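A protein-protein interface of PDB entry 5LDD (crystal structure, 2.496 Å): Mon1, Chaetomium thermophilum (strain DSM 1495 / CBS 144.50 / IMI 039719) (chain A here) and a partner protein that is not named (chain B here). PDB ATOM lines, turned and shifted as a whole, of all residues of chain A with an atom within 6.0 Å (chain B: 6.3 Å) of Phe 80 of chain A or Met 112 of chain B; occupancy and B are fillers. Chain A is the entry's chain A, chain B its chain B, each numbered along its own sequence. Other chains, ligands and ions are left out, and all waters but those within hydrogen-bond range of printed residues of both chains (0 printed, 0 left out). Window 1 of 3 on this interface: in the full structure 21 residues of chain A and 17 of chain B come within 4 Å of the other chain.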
ATOM      1  N   ILE A  66     -19.374   9.125  11.481  1.00  0.00           N
ATOM      2  CA  ILE A  66     -18.186   8.380  11.882  1.00  0.00           C
ATOM      3  C   ILE A  66     -18.551   6.943  12.208  1.00  0.00           C
ATOM      4  O   ILE A  66     -17.866   5.994  11.801  1.00  0.00           O
ATOM      5  CB  ILE A  66     -17.505   9.060  13.082  1.00  0.00           C
ATOM      6  CG1 ILE A  66     -16.869  10.382  12.666  1.00  0.00           C
ATOM      7  CG2 ILE A  66     -16.499   8.126  13.705  1.00  0.00           C
ATOM      8  CD1 ILE A  66     -16.284  11.147  13.824  1.00  0.00           C
ATOM      9  N   TYR A  70     -17.723   2.789   9.966  1.00  0.00           N
ATOM     10  CA  TYR A  70     -17.361   1.481  10.487  1.00  0.00           C
ATOM     11  C   TYR A  70     -18.491   0.472  10.329  1.00  0.00           C
ATOM     12  O   TYR A  70     -18.221  -0.714  10.102  1.00  0.00           O
ATOM     13  CB  TYR A  70     -16.934   1.618  11.941  1.00  0.00           C
ATOM     14  CG  TYR A  70     -15.620   2.340  12.087  1.00  0.00           C
ATOM     15  CD1 TYR A  70     -14.411   1.674  11.879  1.00  0.00           C
ATOM     16  CD2 TYR A  70     -15.578   3.680  12.440  1.00  0.00           C
ATOM     17  CE1 TYR A  70     -13.199   2.325  12.018  1.00  0.00           C
ATOM     18  CE2 TYR A  70     -14.374   4.339  12.582  1.00  0.00           C
ATOM     19  CZ  TYR A  70     -13.189   3.657  12.370  1.00  0.00           C
ATOM     20  OH  TYR A  70     -11.994   4.319  12.511  1.00  0.00           O
ATOM     21  N   LEU A  77     -17.525   0.330  15.471  1.00  0.00           N
ATOM     22  CA  LEU A  77     -16.658   1.209  16.243  1.00  0.00           C
ATOM     23  C   LEU A  77     -17.001   1.107  17.726  1.00  0.00           C
ATOM     24  O   LEU A  77     -18.136   1.388  18.126  1.00  0.00           O
ATOM     25  CB  LEU A  77     -16.817   2.647  15.761  1.00  0.00           C
ATOM     26  CG  LEU A  77     -16.131   3.718  16.598  1.00  0.00           C
ATOM     27  CD1 LEU A  77     -14.625   3.519  16.553  1.00  0.00           C
ATOM     28  CD2 LEU A  77     -16.491   5.098  16.081  1.00  0.00           C
ATOM     29  N   LEU A  78     -16.009   0.744  18.542  1.00  0.00           N
ATOM     30  CA  LEU A  78     -16.185   0.608  19.983  1.00  0.00           C
ATOM     31  C   LEU A  78     -15.795   1.858  20.757  1.00  0.00           C
ATOM     32  O   LEU A  78     -16.434   2.170  21.770  1.00  0.00           O
ATOM     33  CB  LEU A  78     -15.370  -0.576  20.510  1.00  0.00           C
ATOM     34  CG  LEU A  78     -15.713  -1.924  19.864  1.00  0.00           C
ATOM     35  CD1 LEU A  78     -14.828  -3.046  20.397  1.00  0.00           C
ATOM     36  CD2 LEU A  78     -17.191  -2.241  20.082  1.00  0.00           C
ATOM     37  N   GLY A  79     -14.784   2.587  20.307  1.00  0.00           N
ATOM     38  CA  GLY A  79     -14.385   3.796  20.999  1.00  0.00           C
ATOM     39  C   GLY A  79     -13.035   4.259  20.512  1.00  0.00           C
ATOM     40  O   GLY A  79     -12.362   3.585  19.728  1.00  0.00           O
ATOM     41  N   PHE A  80     -12.645   5.440  20.989  1.00  0.00           N
ATOM     42  CA  PHE A  80     -11.342   5.978  20.630  1.00  0.00           C
ATOM     43  C   PHE A  80     -10.892   6.975  21.692  1.00  0.00           C
ATOM     44  O   PHE A  80     -11.656   7.366  22.578  1.00  0.00           O
ATOM     45  CB  PHE A  80     -11.356   6.595  19.218  1.00  0.00           C
ATOM     46  CG  PHE A  80     -12.400   7.638  19.005  1.00  0.00           C
ATOM     47  CD1 PHE A  80     -13.686   7.287  18.619  1.00  0.00           C
ATOM     48  CD2 PHE A  80     -12.084   8.985  19.130  1.00  0.00           C
ATOM     49  CE1 PHE A  80     -14.651   8.263  18.389  1.00  0.00           C
ATOM     50  CE2 PHE A  80     -13.044   9.966  18.898  1.00  0.00           C
ATOM     51  CZ  PHE A  80     -14.329   9.604  18.535  1.00  0.00           C
ATOM     52  N   THR A  81      -9.613   7.350  21.612  1.00  0.00           N
ATOM     53  CA  THR A  81      -8.939   8.135  22.633  1.00  0.00           C
ATOM     54  C   THR A  81      -8.191   9.284  21.986  1.00  0.00           C
ATOM     55  O   THR A  81      -7.496   9.090  20.983  1.00  0.00           O
ATOM     56  CB  THR A  81      -7.942   7.276  23.443  1.00  0.00           C
ATOM     57  OG1 THR A  81      -8.660   6.314  24.227  1.00  0.00           O
ATOM     58  CG2 THR A  81      -7.115   8.145  24.361  1.00  0.00           C
ATOM     59  N   ALA A  82      -8.304  10.467  22.577  1.00  0.00           N
ATOM     60  CA  ALA A  82      -7.587  11.644  22.099  1.00  0.00           C
ATOM     61  C   ALA A  82      -7.053  12.379  23.311  1.00  0.00           C
ATOM     62  O   ALA A  82      -7.827  13.008  24.038  1.00  0.00           O
ATOM     63  CB  ALA A  82      -8.496  12.559  21.269  1.00  0.00           C
ATOM     64  N   VAL A  85      -8.976  12.463  26.749  1.00  0.00           N
ATOM     65  CA  VAL A  85     -10.403  12.261  26.530  1.00  0.00           C
ATOM     66  C   VAL A  85     -10.676  10.877  25.942  1.00  0.00           C
ATOM     67  O   VAL A  85      -9.989  10.425  25.021  1.00  0.00           O
ATOM     68  CB  VAL A  85     -10.966  13.347  25.605  1.00  0.00           C
ATOM     69  CG1 VAL A  85     -12.458  13.169  25.444  1.00  0.00           C
ATOM     70  CG2 VAL A  85     -10.630  14.728  26.157  1.00  0.00           C
ATOM     71  N   ARG A  86     -11.696  10.214  26.468  1.00  0.00           N
ATOM     72  CA  ARG A  86     -12.108   8.917  25.983  1.00  0.00           C
ATOM     73  C   ARG A  86     -13.521   8.994  25.421  1.00  0.00           C
ATOM     74  O   ARG A  86     -14.413   9.603  26.022  1.00  0.00           O
ATOM     75  CB  ARG A  86     -12.013   7.867  27.091  1.00  0.00           C
ATOM     76  CG  ARG A  86     -12.599   6.526  26.707  1.00  0.00           C
ATOM     77  CD  ARG A  86     -12.325   5.446  27.748  1.00  0.00           C
ATOM     78  NE  ARG A  86     -11.331   4.485  27.285  1.00  0.00           N
ATOM     79  CZ  ARG A  86     -10.073   4.431  27.686  1.00  0.00           C
ATOM     80  NH1 ARG A  86      -9.276   3.502  27.178  1.00  0.00           N
ATOM     81  NH2 ARG A  86      -9.617   5.292  28.582  1.00  0.00           N
ATOM     82  N   PHE A  87     -13.708   8.368  24.263  1.00  0.00           N
ATOM     83  CA  PHE A  87     -14.994   8.247  23.595  1.00  0.00           C
ATOM     84  C   PHE A  87     -15.383   6.781  23.592  1.00  0.00           C
ATOM     85  O   PHE A  87     -14.574   5.922  23.223  1.00  0.00           O
ATOM     86  CB  PHE A  87     -14.929   8.749  22.145  1.00  0.00           C
ATOM     87  CG  PHE A  87     -14.472  10.170  22.004  1.00  0.00           C
ATOM     88  CD1 PHE A  87     -13.144  10.521  22.223  1.00  0.00           C
ATOM     89  CD2 PHE A  87     -15.363  11.158  21.620  1.00  0.00           C
ATOM     90  CE1 PHE A  87     -12.718  11.840  22.073  1.00  0.00           C
ATOM     91  CE2 PHE A  87     -14.942  12.478  21.465  1.00  0.00           C
ATOM     92  CZ  PHE A  87     -13.622  12.820  21.689  1.00  0.00           C
ATOM     93  N   VAL A  88     -16.613   6.498  23.993  1.00  0.00           N
ATOM     94  CA  VAL A  88     -17.144   5.144  24.008  1.00  0.00           C
ATOM     95  C   VAL A  88     -18.449   5.144  23.233  1.00  0.00           C
ATOM     96  O   VAL A  88     -19.261   6.066  23.379  1.00  0.00           O
ATOM     97  CB  VAL A  88     -17.336   4.626  25.438  1.00  0.00           C
ATOM     98  CG1 VAL A  88     -18.214   3.389  25.446  1.00  0.00           C
ATOM     99  CG2 VAL A  88     -15.970   4.319  26.027  1.00  0.00           C
ATOM    100  N   ILE A  89     -18.611   4.154  22.358  1.00  0.00           N
ATOM    101  CA  ILE A  89     -19.785   4.012  21.510  1.00  0.00           C
ATOM    102  C   ILE A  89     -20.539   2.773  21.950  1.00  0.00           C
ATOM    103  O   ILE A  89     -19.937   1.709  22.131  1.00  0.00           O
ATOM    104  CB  ILE A  89     -19.401   3.893  20.028  1.00  0.00           C
ATOM    105  CG1 ILE A  89     -18.435   5.016  19.613  1.00  0.00           C
ATOM    106  CG2 ILE A  89     -20.648   3.929  19.178  1.00  0.00           C
ATOM    107  CD1 ILE A  89     -19.049   6.383  19.608  1.00  0.00           C
ATOM    108  N   GLY B 107      -9.270   9.985   5.036  1.00  0.00           N
ATOM    109  CA  GLY B 107     -10.201  11.058   5.354  1.00  0.00           C
ATOM    110  C   GLY B 107     -10.904  10.834   6.684  1.00  0.00           C
ATOM    111  O   GLY B 107     -11.045  11.755   7.492  1.00  0.00           O
ATOM    112  N   LEU B 108     -11.328   9.597   6.941  1.00  0.00           N
ATOM    113  CA  LEU B 108     -11.971   9.297   8.212  1.00  0.00           C
ATOM    114  C   LEU B 108     -11.030   9.583   9.375  1.00  0.00           C
ATOM    115  O   LEU B 108     -11.446  10.140  10.393  1.00  0.00           O
ATOM    116  CB  LEU B 108     -12.434   7.841   8.231  1.00  0.00           C
ATOM    117  CG  LEU B 108     -13.075   7.352   9.526  1.00  0.00           C
ATOM    118  CD1 LEU B 108     -14.470   7.922   9.694  1.00  0.00           C
ATOM    119  CD2 LEU B 108     -13.101   5.830   9.606  1.00  0.00           C
ATOM    120  N   ALA B 109      -9.744   9.262   9.226  1.00  0.00           N
ATOM    121  CA  ALA B 109      -8.803   9.559  10.302  1.00  0.00           C
ATOM    122  C   ALA B 109      -8.724  11.058  10.556  1.00  0.00           C
ATOM    123  O   ALA B 109      -8.730  11.503  11.712  1.00  0.00           O
ATOM    124  CB  ALA B 109      -7.420   9.005   9.971  1.00  0.00           C
ATOM    125  N   GLN B 110      -8.653  11.855   9.490  1.00  0.00           N
ATOM    126  CA  GLN B 110      -8.601  13.304   9.665  1.00  0.00           C
ATOM    127  C   GLN B 110      -9.890  13.835  10.269  1.00  0.00           C
ATOM    128  O   GLN B 110      -9.859  14.727  11.125  1.00  0.00           O
ATOM    129  CB  GLN B 110      -8.327  13.987   8.329  1.00  0.00           C
ATOM    130  CG  GLN B 110      -6.953  13.700   7.745  1.00  0.00           C
ATOM    131  CD  GLN B 110      -6.790  14.332   6.381  1.00  0.00           C
ATOM    132  OE1 GLN B 110      -6.396  13.666   5.415  1.00  0.00           O
ATOM    133  NE2 GLN B 110      -7.090  15.631   6.288  1.00  0.00           N
ATOM    134  N   GLY B 111     -11.035  13.301   9.830  1.00  0.00           N
ATOM    135  CA  GLY B 111     -12.303  13.743  10.392  1.00  0.00           C
ATOM    136  C   GLY B 111     -12.402  13.440  11.878  1.00  0.00           C
ATOM    137  O   GLY B 111     -12.860  14.272  12.665  1.00  0.00           O
ATOM    138  N   MET B 112     -11.953  12.254  12.288  1.00  0.00           N
ATOM    139  CA  MET B 112     -11.980  11.940  13.709  1.00  0.00           C
ATOM    140  C   MET B 112     -11.036  12.841  14.492  1.00  0.00           C
ATOM    141  O   MET B 112     -11.349  13.250  15.612  1.00  0.00           O
ATOM    142  CB  MET B 112     -11.671  10.472  13.928  1.00  0.00           C
ATOM    143  CG  MET B 112     -12.771   9.612  13.361  1.00  0.00           C
ATOM    144  SD  MET B 112     -12.404   7.859  13.493  1.00  0.00           S
ATOM    145  CE  MET B 112     -12.631   7.532  15.243  1.00  0.00           C
ATOM    146  N   VAL B 113      -9.884  13.177  13.905  1.00  0.00           N
ATOM    147  CA  VAL B 113      -8.966  14.130  14.518  1.00  0.00           C
ATOM    148  C   VAL B 113      -9.633  15.488  14.688  1.00  0.00           C
ATOM    149  O   VAL B 113      -9.632  16.073  15.779  1.00  0.00           O
ATOM    150  CB  VAL B 113      -7.690  14.247  13.668  1.00  0.00           C
ATOM    151  CG1 VAL B 113      -6.874  15.470  14.084  1.00  0.00           C
ATOM    152  CG2 VAL B 113      -6.889  12.992  13.805  1.00  0.00           C
ATOM    153  N   GLU B 114     -10.217  16.010  13.605  1.00  0.00           N
ATOM    154  CA  GLU B 114     -10.893  17.305  13.674  1.00  0.00           C
ATOM    155  C   GLU B 114     -12.014  17.286  14.701  1.00  0.00           C
ATOM    156  O   GLU B 114     -12.158  18.221  15.496  1.00  0.00           O
ATOM    157  CB  GLU B 114     -11.446  17.682  12.301  1.00  0.00           C
ATOM    158  CG  GLU B 114     -12.042  19.055  12.231  1.00  0.00           C
ATOM    159  CD  GLU B 114     -11.024  20.130  12.549  1.00  0.00           C
ATOM    160  OE1 GLU B 114     -11.417  21.181  13.101  1.00  0.00           O
ATOM    161  OE2 GLU B 114      -9.830  19.924  12.237  1.00  0.00           O
ATOM    162  N   PHE B 115     -12.788  16.204  14.733  1.00  0.00           N
ATOM    163  CA  PHE B 115     -13.908  16.122  15.657  1.00  0.00           C
ATOM    164  C   PHE B 115     -13.426  16.086  17.103  1.00  0.00           C
ATOM    165  O   PHE B 115     -13.894  16.860  17.947  1.00  0.00           O
ATOM    166  CB  PHE B 115     -14.748  14.889  15.324  1.00  0.00           C
ATOM    167  CG  PHE B 115     -15.753  14.541  16.371  1.00  0.00           C
ATOM    168  CD1 PHE B 115     -16.921  15.261  16.486  1.00  0.00           C
ATOM    169  CD2 PHE B 115     -15.519  13.490  17.251  1.00  0.00           C
ATOM    170  CE1 PHE B 115     -17.853  14.938  17.460  1.00  0.00           C
ATOM    171  CE2 PHE B 115     -16.450  13.163  18.235  1.00  0.00           C
ATOM    172  CZ  PHE B 115     -17.616  13.887  18.336  1.00  0.00           C
ATOM    173  N   ALA B 116     -12.467  15.217  17.403  1.00  0.00           N
ATOM    174  CA  ALA B 116     -12.019  15.076  18.783  1.00  0.00           C
ATOM    175  C   ALA B 116     -11.255  16.298  19.283  1.00  0.00           C
ATOM    176  O   ALA B 116     -11.263  16.559  20.489  1.00  0.00           O
ATOM    177  CB  ALA B 116     -11.161  13.818  18.934  1.00  0.00           C
ATOM    178  N   LYS B 117     -10.637  17.083  18.397  1.00  0.00           N
ATOM    179  CA  LYS B 117      -9.898  18.255  18.869  1.00  0.00           C
ATOM    180  C   LYS B 117     -10.802  19.240  19.606  1.00  0.00           C
ATOM    181  O   LYS B 117     -10.327  19.986  20.470  1.00  0.00           O
ATOM    182  CB  LYS B 117      -9.185  18.946  17.709  1.00  0.00           C
ATOM    183  CG  LYS B 117      -7.800  18.385  17.408  1.00  0.00           C
ATOM    184  CD  LYS B 117      -7.161  19.087  16.220  1.00  0.00           C
ATOM    185  CE  LYS B 117      -5.755  18.566  15.971  1.00  0.00           C
ATOM    186  NZ  LYS B 117      -5.198  19.085  14.684  1.00  0.00           N
ATOM    187  N   VAL B 125      -6.647  12.299  17.862  1.00  0.00           N
ATOM    188  CA  VAL B 125      -6.935  10.894  18.112  1.00  0.00           C
ATOM    189  C   VAL B 125      -5.651  10.098  17.930  1.00  0.00           C
ATOM    190  O   VAL B 125      -4.930  10.274  16.939  1.00  0.00           O
ATOM    191  CB  VAL B 125      -8.029  10.400  17.152  1.00  0.00           C
ATOM    192  CG1 VAL B 125      -8.276   8.921  17.350  1.00  0.00           C
ATOM    193  CG2 VAL B 125      -9.301  11.186  17.349  1.00  0.00           C
ATOM    194  N   THR B 127      -5.654   6.475  19.220  1.00  0.00           N
ATOM    195  CA  THR B 127      -6.036   5.072  19.284  1.00  0.00           C
ATOM    196  C   THR B 127      -7.512   4.933  18.940  1.00  0.00           C
ATOM    197  O   THR B 127      -8.344   5.693  19.446  1.00  0.00           O
ATOM    198  CB  THR B 127      -5.793   4.506  20.688  1.00  0.00           C
ATOM    199  OG1 THR B 127      -4.435   4.747  21.067  1.00  0.00           O
ATOM    200  CG2 THR B 127      -6.072   3.024  20.708  1.00  0.00           C
ATOM    201  N   ILE B 128      -7.841   3.961  18.099  1.00  0.00           N
ATOM    202  CA  ILE B 128      -9.225   3.659  17.747  1.00  0.00           C
ATOM    203  C   ILE B 128      -9.447   2.173  17.961  1.00  0.00           C
ATOM    204  O   ILE B 128      -8.662   1.350  17.470  1.00  0.00           O
ATOM    205  CB  ILE B 128      -9.537   4.051  16.290  1.00  0.00           C
ATOM    206  CG1 ILE B 128      -9.270   5.553  16.091  1.00  0.00           C
ATOM    207  CG2 ILE B 128     -10.967   3.660  15.927  1.00  0.00           C
ATOM    208  CD1 ILE B 128      -9.276   5.998  14.645  1.00  0.00           C
ATOM    209  N   ASP B 129     -10.503   1.827  18.693  1.00  0.00           N
ATOM    210  CA  ASP B 129     -10.805   0.437  19.006  1.00  0.00           C
ATOM    211  C   ASP B 129     -12.054   0.017  18.244  1.00  0.00           C
ATOM    212  O   ASP B 129     -13.135   0.579  18.459  1.00  0.00           O
ATOM    213  CB  ASP B 129     -10.980   0.253  20.511  1.00  0.00           C
ATOM    214  CG  ASP B 129      -9.705   0.575  21.283  1.00  0.00           C
ATOM    215  OD1 ASP B 129      -8.770  -0.258  21.248  1.00  0.00           O
ATOM    216  OD2 ASP B 129      -9.635   1.655  21.919  1.00  0.00           O
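N of Ile 89 of chain A is in hydrogen-bond range of O of Leu 78 of chain A (3.0 Å).
The backbone carbonyl oxygen of Phe 80 of chain A sits at hydrogen-bond distance from the backbone NH of Phe 87 of chain A (2.8 Å).
Tyr 70 of chain A touches Ile 128 of chain B.
CD1 of Leu 77 of chain A touches O of Asp 129 of chain B, at 3.8 Å.
Gly 79 of chain A touches Ile 128 of chain B (O to C, 3.7 Å).
Phe 80 of chain A touches Met 112 of chain B (CD1 to CE, 3.5 Å).
CB of Phe 80 of chain A touches O of Thr 127 of chain B, 3.2 Å away.
Phe 80 of chain A touches Ile 128 of chain B (CB to CG1, 3.9 Å).
Ala 116 of chain B touches Ala 82 of chain A.
CB of Ala 82 of chain A touches N of Val 125 of chain B, 3.9 Å away.
CE2 of Phe 115 of chain B touches CE2 of Phe 87 of chain A (3.6 Å).
CB of Ala 116 of chain B touches CZ of Phe 87 of chain A (3.8 Å).
Of the printed residues of chain A, Met 112 of chain B touches Ile 66, Tyr 70 and Phe 80.
Printed residues of chain B within 4 Å of Ile 66 of chain A: Met 112 (3.9 Å).
Of the printed residues of chain A, Thr 127 of chain B touches Phe 80 (3.2 Å) and Thr 81 (3.0 Å).
Of the printed residues of chain B, Tyr 70 of chain A touches Leu 108 (3.5 Å), Met 112 (3.7 Å) and Ile 128 (3.6 Å).
Printed residues of chain B within 4 Å of Thr 81 of chain A: Val 125 (3.4 Å) and Thr 127 (3.0 Å).
Of the printed residues of chain B, Leu 77 of chain A touches Ile 128 and Asp 129.
Lys 117 of chain B touches none of the printed residues of chain A.
The nearest residue of chain B that does not touch Phe 80 of chain A is Phe 115 of chain B (4.2 Å).
Of the 15 printed residues of chain B, 8 touch a printed residue of chain A.
Hydrophobic or aromatic side chains of chain B that line the printed part of chain A: Leu 108, Met 112, Phe 115, Ala 116, Val 125 and Ile 128.
Of the 13 printed residues of chain A, 9 touch a printed residue of chain B.
Hydrophobic or aromatic side chains of chain A within 4 Å of the printed part of chain B: Ile 66, Tyr 70, Leu 77, Leu 78, Phe 80, Ala 82 and Phe 87.
Among the printed residues, 19 pairs touch across the chains.
Among the printed residues, no Asp or Glu carboxylate lies within 4 Å of a Lys or Arg side-chain nitrogen of the other chain.
The side-chain hydroxyl of Tyr 70 of chain A lies within hydrogen-bond range of the side-chain sulfur of Met 112 of chain B, 3.7 Å away.
N of Leu 78 of chain A is in hydrogen-bond range of O of Asp 129 of chain B, 2.9 Å away.
The backbone carbonyl oxygen (O) of Gly 79 of chain A sits at hydrogen-bond distance from the backbone NH (N) of Asp 129 of chain B, 2.8 Å away.
The backbone NH (N) of Thr 81 of chain A lies within hydrogen-bond range of the backbone carbonyl oxygen (O) of Thr 127 of chain B, 3.0 Å away.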
